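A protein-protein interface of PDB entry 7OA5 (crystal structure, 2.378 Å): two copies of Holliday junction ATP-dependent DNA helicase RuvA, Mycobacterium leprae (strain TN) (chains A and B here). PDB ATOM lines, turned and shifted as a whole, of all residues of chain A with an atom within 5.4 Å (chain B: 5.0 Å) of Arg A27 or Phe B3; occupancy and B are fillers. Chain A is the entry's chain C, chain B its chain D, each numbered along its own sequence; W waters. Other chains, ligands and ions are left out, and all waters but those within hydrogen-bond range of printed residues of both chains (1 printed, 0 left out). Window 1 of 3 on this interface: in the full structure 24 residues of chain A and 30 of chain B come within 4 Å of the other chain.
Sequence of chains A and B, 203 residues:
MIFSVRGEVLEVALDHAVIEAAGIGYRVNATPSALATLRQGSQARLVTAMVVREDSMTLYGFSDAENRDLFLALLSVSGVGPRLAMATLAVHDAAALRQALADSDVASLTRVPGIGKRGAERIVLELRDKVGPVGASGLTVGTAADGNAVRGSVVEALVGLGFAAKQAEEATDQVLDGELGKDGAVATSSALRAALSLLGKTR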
ATOM      1  N   ASP A  15      22.624   9.391 -12.709  1.00  0.00           N
ATOM      2  CA  ASP A  15      21.774  10.349 -11.993  1.00  0.00           C
ATOM      3  C   ASP A  15      20.886   9.752 -10.896  1.00  0.00           C
ATOM      4  O   ASP A  15      20.139  10.480 -10.223  1.00  0.00           O
ATOM      5  CB  ASP A  15      20.911  11.140 -12.986  1.00  0.00           C
ATOM      6  CG  ASP A  15      19.859  10.318 -13.695  1.00  0.00           C
ATOM      7  OD1 ASP A  15      20.021   9.081 -13.773  1.00  0.00           O
ATOM      8  OD2 ASP A  15      18.877  10.915 -14.193  1.00  0.00           O
ATOM      9  N   HIS A  16      20.945   8.433 -10.718  1.00  0.00           N
ATOM     10  CA  HIS A  16      20.125   7.766  -9.719  1.00  0.00           C
ATOM     11  C   HIS A  16      20.682   6.390  -9.397  1.00  0.00           C
ATOM     12  O   HIS A  16      21.518   5.857 -10.122  1.00  0.00           O
ATOM     13  CB  HIS A  16      18.650   7.667 -10.222  1.00  0.00           C
ATOM     14  CG  HIS A  16      18.415   6.576 -11.215  1.00  0.00           C
ATOM     15  ND1 HIS A  16      18.693   6.753 -12.571  1.00  0.00           N
ATOM     16  CD2 HIS A  16      17.931   5.323 -11.026  1.00  0.00           C
ATOM     17  CE1 HIS A  16      18.385   5.602 -13.153  1.00  0.00           C
ATOM     18  NE2 HIS A  16      17.938   4.706 -12.262  1.00  0.00           N
ATOM     19  N   ALA A  17      20.177   5.796  -8.333  1.00  0.00           N
ATOM     20  CA  ALA A  17      20.481   4.418  -7.965  1.00  0.00           C
ATOM     21  C   ALA A  17      19.173   3.762  -7.521  1.00  0.00           C
ATOM     22  O   ALA A  17      18.221   4.448  -7.148  1.00  0.00           O
ATOM     23  CB  ALA A  17      21.494   4.367  -6.826  1.00  0.00           C
ATOM     24  N   VAL A  18      19.110   2.443  -7.596  1.00  0.00           N
ATOM     25  CA  VAL A  18      17.992   1.697  -7.064  1.00  0.00           C
ATOM     26  C   VAL A  18      18.560   0.941  -5.878  1.00  0.00           C
ATOM     27  O   VAL A  18      19.563   0.247  -6.024  1.00  0.00           O
ATOM     28  CB  VAL A  18      17.288   0.769  -8.082  1.00  0.00           C
ATOM     29  CG1 VAL A  18      16.162  -0.005  -7.402  1.00  0.00           C
ATOM     30  CG2 VAL A  18      16.758   1.566  -9.279  1.00  0.00           C
ATOM     31  N   ILE A  19      17.996   1.148  -4.693  1.00  0.00           N
ATOM     32  CA  ILE A  19      18.452   0.489  -3.480  1.00  0.00           C
ATOM     33  C   ILE A  19      17.306  -0.337  -2.930  1.00  0.00           C
ATOM     34  O   ILE A  19      16.233   0.195  -2.685  1.00  0.00           O
ATOM     35  CB  ILE A  19      18.955   1.530  -2.443  1.00  0.00           C
ATOM     36  CG1 ILE A  19      20.141   2.330  -3.030  1.00  0.00           C
ATOM     37  CG2 ILE A  19      19.352   0.833  -1.149  1.00  0.00           C
ATOM     38  CD1 ILE A  19      20.686   3.390  -2.169  1.00  0.00           C
ATOM     39  N   GLY A  25      12.723  -2.069  -4.034  1.00  0.00           N
ATOM     40  CA  GLY A  25      13.756  -1.303  -4.699  1.00  0.00           C
ATOM     41  C   GLY A  25      13.307   0.141  -4.801  1.00  0.00           C
ATOM     42  O   GLY A  25      12.293   0.423  -5.414  1.00  0.00           O
ATOM     43  N   TYR A  26      14.012   1.051  -4.145  1.00  0.00           N
ATOM     44  CA  TYR A  26      13.680   2.463  -4.168  1.00  0.00           C
ATOM     45  C   TYR A  26      14.546   3.150  -5.175  1.00  0.00           C
ATOM     46  O   TYR A  26      15.758   2.981  -5.138  1.00  0.00           O
ATOM     47  CB  TYR A  26      13.941   3.096  -2.800  1.00  0.00           C
ATOM     48  CG  TYR A  26      12.959   2.624  -1.764  1.00  0.00           C
ATOM     49  CD1 TYR A  26      11.731   3.246  -1.612  1.00  0.00           C
ATOM     50  CD2 TYR A  26      13.222   1.504  -0.993  1.00  0.00           C
ATOM     51  CE1 TYR A  26      10.801   2.788  -0.693  1.00  0.00           C
ATOM     52  CE2 TYR A  26      12.306   1.044  -0.059  1.00  0.00           C
ATOM     53  CZ  TYR A  26      11.097   1.692   0.091  1.00  0.00           C
ATOM     54  OH  TYR A  26      10.179   1.230   0.995  1.00  0.00           O
ATOM     55  N   ARG A  27      13.939   3.921  -6.070  1.00  0.00           N
ATOM     56  CA  ARG A  27      14.687   4.715  -7.002  1.00  0.00           C
ATOM     57  C   ARG A  27      15.029   5.960  -6.208  1.00  0.00           C
ATOM     58  O   ARG A  27      14.154   6.597  -5.607  1.00  0.00           O
ATOM     59  CB  ARG A  27      13.889   5.082  -8.248  1.00  0.00           C
ATOM     60  CG  ARG A  27      14.765   5.838  -9.242  1.00  0.00           C
ATOM     61  CD  ARG A  27      13.923   6.600 -10.241  1.00  0.00           C
ATOM     62  NE  ARG A  27      14.682   7.667 -10.906  1.00  0.00           N
ATOM     63  CZ  ARG A  27      15.162   7.590 -12.138  1.00  0.00           C
ATOM     64  NH1 ARG A  27      15.005   6.483 -12.851  1.00  0.00           N
ATOM     65  NH2 ARG A  27      15.824   8.611 -12.661  1.00  0.00           N
ATOM     66  N   VAL A  28      16.319   6.289  -6.169  1.00  0.00           N
ATOM     67  CA  VAL A  28      16.787   7.451  -5.450  1.00  0.00           C
ATOM     68  C   VAL A  28      17.560   8.293  -6.425  1.00  0.00           C
ATOM     69  O   VAL A  28      18.613   7.862  -6.882  1.00  0.00           O
ATOM     70  CB  VAL A  28      17.662   7.058  -4.234  1.00  0.00           C
ATOM     71  CG1 VAL A  28      18.042   8.293  -3.452  1.00  0.00           C
ATOM     72  CG2 VAL A  28      16.951   6.042  -3.317  1.00  0.00           C
ATOM     73  N   ASN A  29      17.038   9.479  -6.775  1.00  0.00           N
ATOM     74  CA  ASN A  29      17.732  10.427  -7.654  1.00  0.00           C
ATOM     75  C   ASN A  29      18.847  10.999  -6.835  1.00  0.00           C
ATOM     76  O   ASN A  29      18.570  11.553  -5.797  1.00  0.00           O
ATOM     77  CB  ASN A  29      16.794  11.535  -8.046  1.00  0.00           C
ATOM     78  CG  ASN A  29      15.694  11.024  -8.918  1.00  0.00           C
ATOM     79  OD1 ASN A  29      15.864  10.088  -9.705  1.00  0.00           O
ATOM     80  ND2 ASN A  29      14.542  11.628  -8.817  1.00  0.00           N
ATOM     81  N   LEU A  59      12.403  10.211  -4.157  1.00  0.00           N
ATOM     82  CA  LEU A  59      13.494  10.243  -3.203  1.00  0.00           C
ATOM     83  C   LEU A  59      14.693  10.887  -3.865  1.00  0.00           C
ATOM     84  O   LEU A  59      15.025  10.585  -5.011  1.00  0.00           O
ATOM     85  CB  LEU A  59      13.876   8.830  -2.745  1.00  0.00           C
ATOM     86  CG  LEU A  59      12.871   8.108  -1.896  1.00  0.00           C
ATOM     87  CD1 LEU A  59      13.290   6.670  -1.709  1.00  0.00           C
ATOM     88  CD2 LEU A  59      12.685   8.803  -0.564  1.00  0.00           C
ATOM     89  N   MET B   1       8.632   5.945  -7.138  1.00  0.00           N
ATOM     90  CA  MET B   1       9.649   5.755  -6.108  1.00  0.00           C
ATOM     91  C   MET B   1      10.014   4.290  -6.013  1.00  0.00           C
ATOM     92  O   MET B   1      11.163   3.964  -5.830  1.00  0.00           O
ATOM     93  CB  MET B   1       9.106   6.298  -4.786  1.00  0.00           C
ATOM     94  CG  MET B   1       9.931   6.002  -3.593  1.00  0.00           C
ATOM     95  SD  MET B   1       9.171   6.901  -2.261  1.00  0.00           S
ATOM     96  CE  MET B   1       8.593   5.594  -1.256  1.00  0.00           C
ATOM     97  N   ILE B   2       9.028   3.410  -6.101  1.00  0.00           N
ATOM     98  CA  ILE B   2       9.233   1.980  -6.049  1.00  0.00           C
ATOM     99  C   ILE B   2       9.601   1.483  -7.436  1.00  0.00           C
ATOM    100  O   ILE B   2       8.800   1.559  -8.361  1.00  0.00           O
ATOM    101  CB  ILE B   2       7.984   1.284  -5.452  1.00  0.00           C
ATOM    102  CG1 ILE B   2       7.766   1.768  -4.007  1.00  0.00           C
ATOM    103  CG2 ILE B   2       8.117  -0.258  -5.541  1.00  0.00           C
ATOM    104  CD1 ILE B   2       6.567   1.052  -3.226  1.00  0.00           C
ATOM    105  N   PHE B   3      10.832   1.024  -7.594  1.00  0.00           N
ATOM    106  CA  PHE B   3      11.320   0.518  -8.865  1.00  0.00           C
ATOM    107  C   PHE B   3      11.316  -0.996  -8.955  1.00  0.00           C
ATOM    108  O   PHE B   3      11.386  -1.530 -10.061  1.00  0.00           O
ATOM    109  CB  PHE B   3      12.693   1.112  -9.228  1.00  0.00           C
ATOM    110  CG  PHE B   3      12.592   2.139 -10.341  1.00  0.00           C
ATOM    111  CD1 PHE B   3      11.443   2.921 -10.495  1.00  0.00           C
ATOM    112  CD2 PHE B   3      13.636   2.321 -11.235  1.00  0.00           C
ATOM    113  CE1 PHE B   3      11.318   3.807 -11.558  1.00  0.00           C
ATOM    114  CE2 PHE B   3      13.525   3.242 -12.279  1.00  0.00           C
ATOM    115  CZ  PHE B   3      12.365   3.974 -12.437  1.00  0.00           C
ATOM    116  N   SER B   4      11.144  -1.700  -7.832  1.00  0.00           N
ATOM    117  CA  SER B   4      10.986  -3.131  -7.852  1.00  0.00           C
ATOM    118  C   SER B   4      10.365  -3.651  -6.566  1.00  0.00           C
ATOM    119  O   SER B   4      10.443  -3.007  -5.528  1.00  0.00           O
ATOM    120  CB  SER B   4      12.293  -3.838  -8.195  1.00  0.00           C
ATOM    121  OG  SER B   4      13.254  -3.636  -7.178  1.00  0.00           O
ATOM    122  N   VAL B   5       9.730  -4.816  -6.651  1.00  0.00           N
ATOM    123  CA  VAL B   5       9.131  -5.475  -5.507  1.00  0.00           C
ATOM    124  C   VAL B   5       9.619  -6.893  -5.550  1.00  0.00           C
ATOM    125  O   VAL B   5       9.467  -7.562  -6.566  1.00  0.00           O
ATOM    126  CB  VAL B   5       7.579  -5.423  -5.511  1.00  0.00           C
ATOM    127  CG1 VAL B   5       7.011  -6.128  -4.268  1.00  0.00           C
ATOM    128  CG2 VAL B   5       7.093  -3.972  -5.611  1.00  0.00           C
ATOM    129  N   LEU B  46       9.825  -8.290  -9.266  1.00  0.00           N
ATOM    130  CA  LEU B  46       9.122  -7.699 -10.369  1.00  0.00           C
ATOM    131  C   LEU B  46       9.592  -6.252 -10.499  1.00  0.00           C
ATOM    132  O   LEU B  46       9.656  -5.527  -9.508  1.00  0.00           O
ATOM    133  CB  LEU B  46       7.627  -7.757 -10.070  1.00  0.00           C
ATOM    134  CG  LEU B  46       6.657  -7.897 -11.237  1.00  0.00           C
ATOM    135  CD1 LEU B  46       7.085  -8.989 -12.243  1.00  0.00           C
ATOM    136  CD2 LEU B  46       5.269  -8.186 -10.707  1.00  0.00           C
ATOM    137  N   VAL B  47       9.952  -5.849 -11.712  1.00  0.00           N
ATOM    138  CA  VAL B  47      10.391  -4.493 -11.979  1.00  0.00           C
ATOM    139  C   VAL B  47       9.130  -3.638 -12.081  1.00  0.00           C
ATOM    140  O   VAL B  47       8.185  -4.056 -12.721  1.00  0.00           O
ATOM    141  CB  VAL B  47      11.233  -4.513 -13.261  1.00  0.00           C
ATOM    142  CG1 VAL B  47      11.431  -3.109 -13.782  1.00  0.00           C
ATOM    143  CG2 VAL B  47      12.576  -5.193 -13.007  1.00  0.00           C
ATOM    144  N   THR B  48       9.054  -2.519 -11.355  1.00  0.00           N
ATOM    145  CA  THR B  48       7.824  -1.748 -11.247  1.00  0.00           C
ATOM    146  C   THR B  48       7.942  -0.248 -11.535  1.00  0.00           C
ATOM    147  O   THR B  48       9.028   0.309 -11.559  1.00  0.00           O
ATOM    148  CB  THR B  48       7.174  -1.949  -9.807  1.00  0.00           C
ATOM    149  OG1 THR B  48       7.985  -1.299  -8.834  1.00  0.00           O
ATOM    150  CG2 THR B  48       6.919  -3.403  -9.421  1.00  0.00           C
ATOM    151  N   ARG B  68       9.520  -1.474 -18.399  1.00  0.00           N
ATOM    152  CA  ARG B  68       9.078  -0.516 -17.416  1.00  0.00           C
ATOM    153  C   ARG B  68       9.345   0.892 -17.909  1.00  0.00           C
ATOM    154  O   ARG B  68       8.488   1.743 -17.754  1.00  0.00           O
ATOM    155  CB  ARG B  68       9.782  -0.750 -16.073  1.00  0.00           C
ATOM    156  CG  ARG B  68       9.202   0.124 -14.975  1.00  0.00           C
ATOM    157  CD  ARG B  68      10.077   1.292 -14.637  1.00  0.00           C
ATOM    158  NE  ARG B  68      10.963   0.831 -13.589  1.00  0.00           N
ATOM    159  CZ  ARG B  68      12.223   0.462 -13.773  1.00  0.00           C
ATOM    160  NH1 ARG B  68      12.805   0.624 -14.953  1.00  0.00           N
ATOM    161  NH2 ARG B  68      12.940   0.009 -12.757  1.00  0.00           N
ATOM    162  N   ASP B  69      10.526   1.131 -18.507  1.00  0.00           N
ATOM    163  CA  ASP B  69      10.902   2.431 -19.054  1.00  0.00           C
ATOM    164  C   ASP B  69      10.036   2.788 -20.264  1.00  0.00           C
ATOM    165  O   ASP B  69       9.673   3.943 -20.426  1.00  0.00           O
ATOM    166  CB  ASP B  69      12.389   2.467 -19.400  1.00  0.00           C
ATOM    167  CG  ASP B  69      13.310   2.379 -18.192  1.00  0.00           C
ATOM    168  OD1 ASP B  69      12.822   2.571 -17.049  1.00  0.00           O
ATOM    169  OD2 ASP B  69      14.517   2.106 -18.386  1.00  0.00           O
ATOM    170  N   LEU B  72       6.733   4.014 -18.896  1.00  0.00           N
ATOM    171  CA  LEU B  72       6.880   5.389 -18.437  1.00  0.00           C
ATOM    172  C   LEU B  72       6.929   6.378 -19.603  1.00  0.00           C
ATOM    173  O   LEU B  72       6.376   7.475 -19.497  1.00  0.00           O
ATOM    174  CB  LEU B  72       8.125   5.513 -17.554  1.00  0.00           C
ATOM    175  CG  LEU B  72       7.993   4.863 -16.175  1.00  0.00           C
ATOM    176  CD1 LEU B  72       9.302   4.906 -15.436  1.00  0.00           C
ATOM    177  CD2 LEU B  72       6.894   5.533 -15.359  1.00  0.00           C
HETATM  178  O   HOH W   1      13.059  -5.283  -5.167  1.00  0.00           O
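Water W1 bridges the side-chain hydroxyl of Ser B4 (2.6 Å) and the backbone NH of Gly A25 (3.4 Å).
Of the 11 printed residues of chain A, 5 touch a printed residue of chain B.
Printed residues of chain A that touch a printed residue of chain B: Val A18, Gly A25, Tyr A26, Arg A27 and Leu A59.
Hydrophobic or aromatic side chains of chain A that line the printed part of chain B: Val A18, Tyr A26 and Leu A59.
Hydrophobic or aromatic side chains of chain B that line the printed part of chain A: Met B1 and Phe B3.
Among the printed residues, 9 pairs touch across the chains.
Among the printed residues, no Asp or Glu carboxylate lies within 4 Å of a Lys or Arg side-chain nitrogen of the other chain.
Among the printed residues, pairs that only touch across the chains: Tyr A26 with Met B1 (3.4 Å), Gly A25 with Ile B2 (3.5 Å), Arg A27 with Phe B3 (3.6 Å), Gly A25 with Met B1 (3.7 Å), Val A18 with Phe B3 (3.8 Å) and Leu A59 with Met B1 (3.9 Å).
O of Gly A25 sits at hydrogen-bond distance from N of Phe B3 (2.7 Å).
The backbone carbonyl oxygen (O) of Met B1 lies within hydrogen-bond range of the backbone NH (N) of Arg A27 (2.8 Å).
The backbone NH (N) of Gly A25 sits at hydrogen-bond distance from the backbone carbonyl oxygen (O) of Ser B4 (2.9 Å).
Of chain B, only Met B1 and Phe B3 come within 4 Å of Arg A27.
Printed residues of chain B within 4 Å of Tyr A26: Met B1.
Of the printed residues of chain A, Ile B2 touches Gly A25 (3.5 Å).
Of the printed residues of chain B, Leu A59 touches Met B1 (3.9 Å).
Asn A29 touches none of the printed residues of chain B.
No position is printed for both chains.
Of the 9 pairs that touch across the chains among the printed residues, none has its exchanged pair printed and touching as well.
A ring nitrogen (ND1) of His A16 is in hydrogen-bond range of the guanidinium group (NH2) of Arg A27 (3.4 Å).
The backbone carbonyl oxygen (O) of Ile B2 is in hydrogen-bond range of the side-chain hydroxyl (OG1) of Thr B48 (3.0 Å).
N of Ser B4 sits at hydrogen-bond distance from OG1 of Thr B48 (3.3 Å).
O of Ile A19 lies within hydrogen-bond range of N of Tyr A26 (2.8 Å).
The backbone NH of Asn A29 lies within hydrogen-bond range of the backbone carbonyl oxygen of Leu A59 (2.9 Å).
OD1 of Asn A29 lies within hydrogen-bond range of NE of Arg A27 (2.9 Å).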
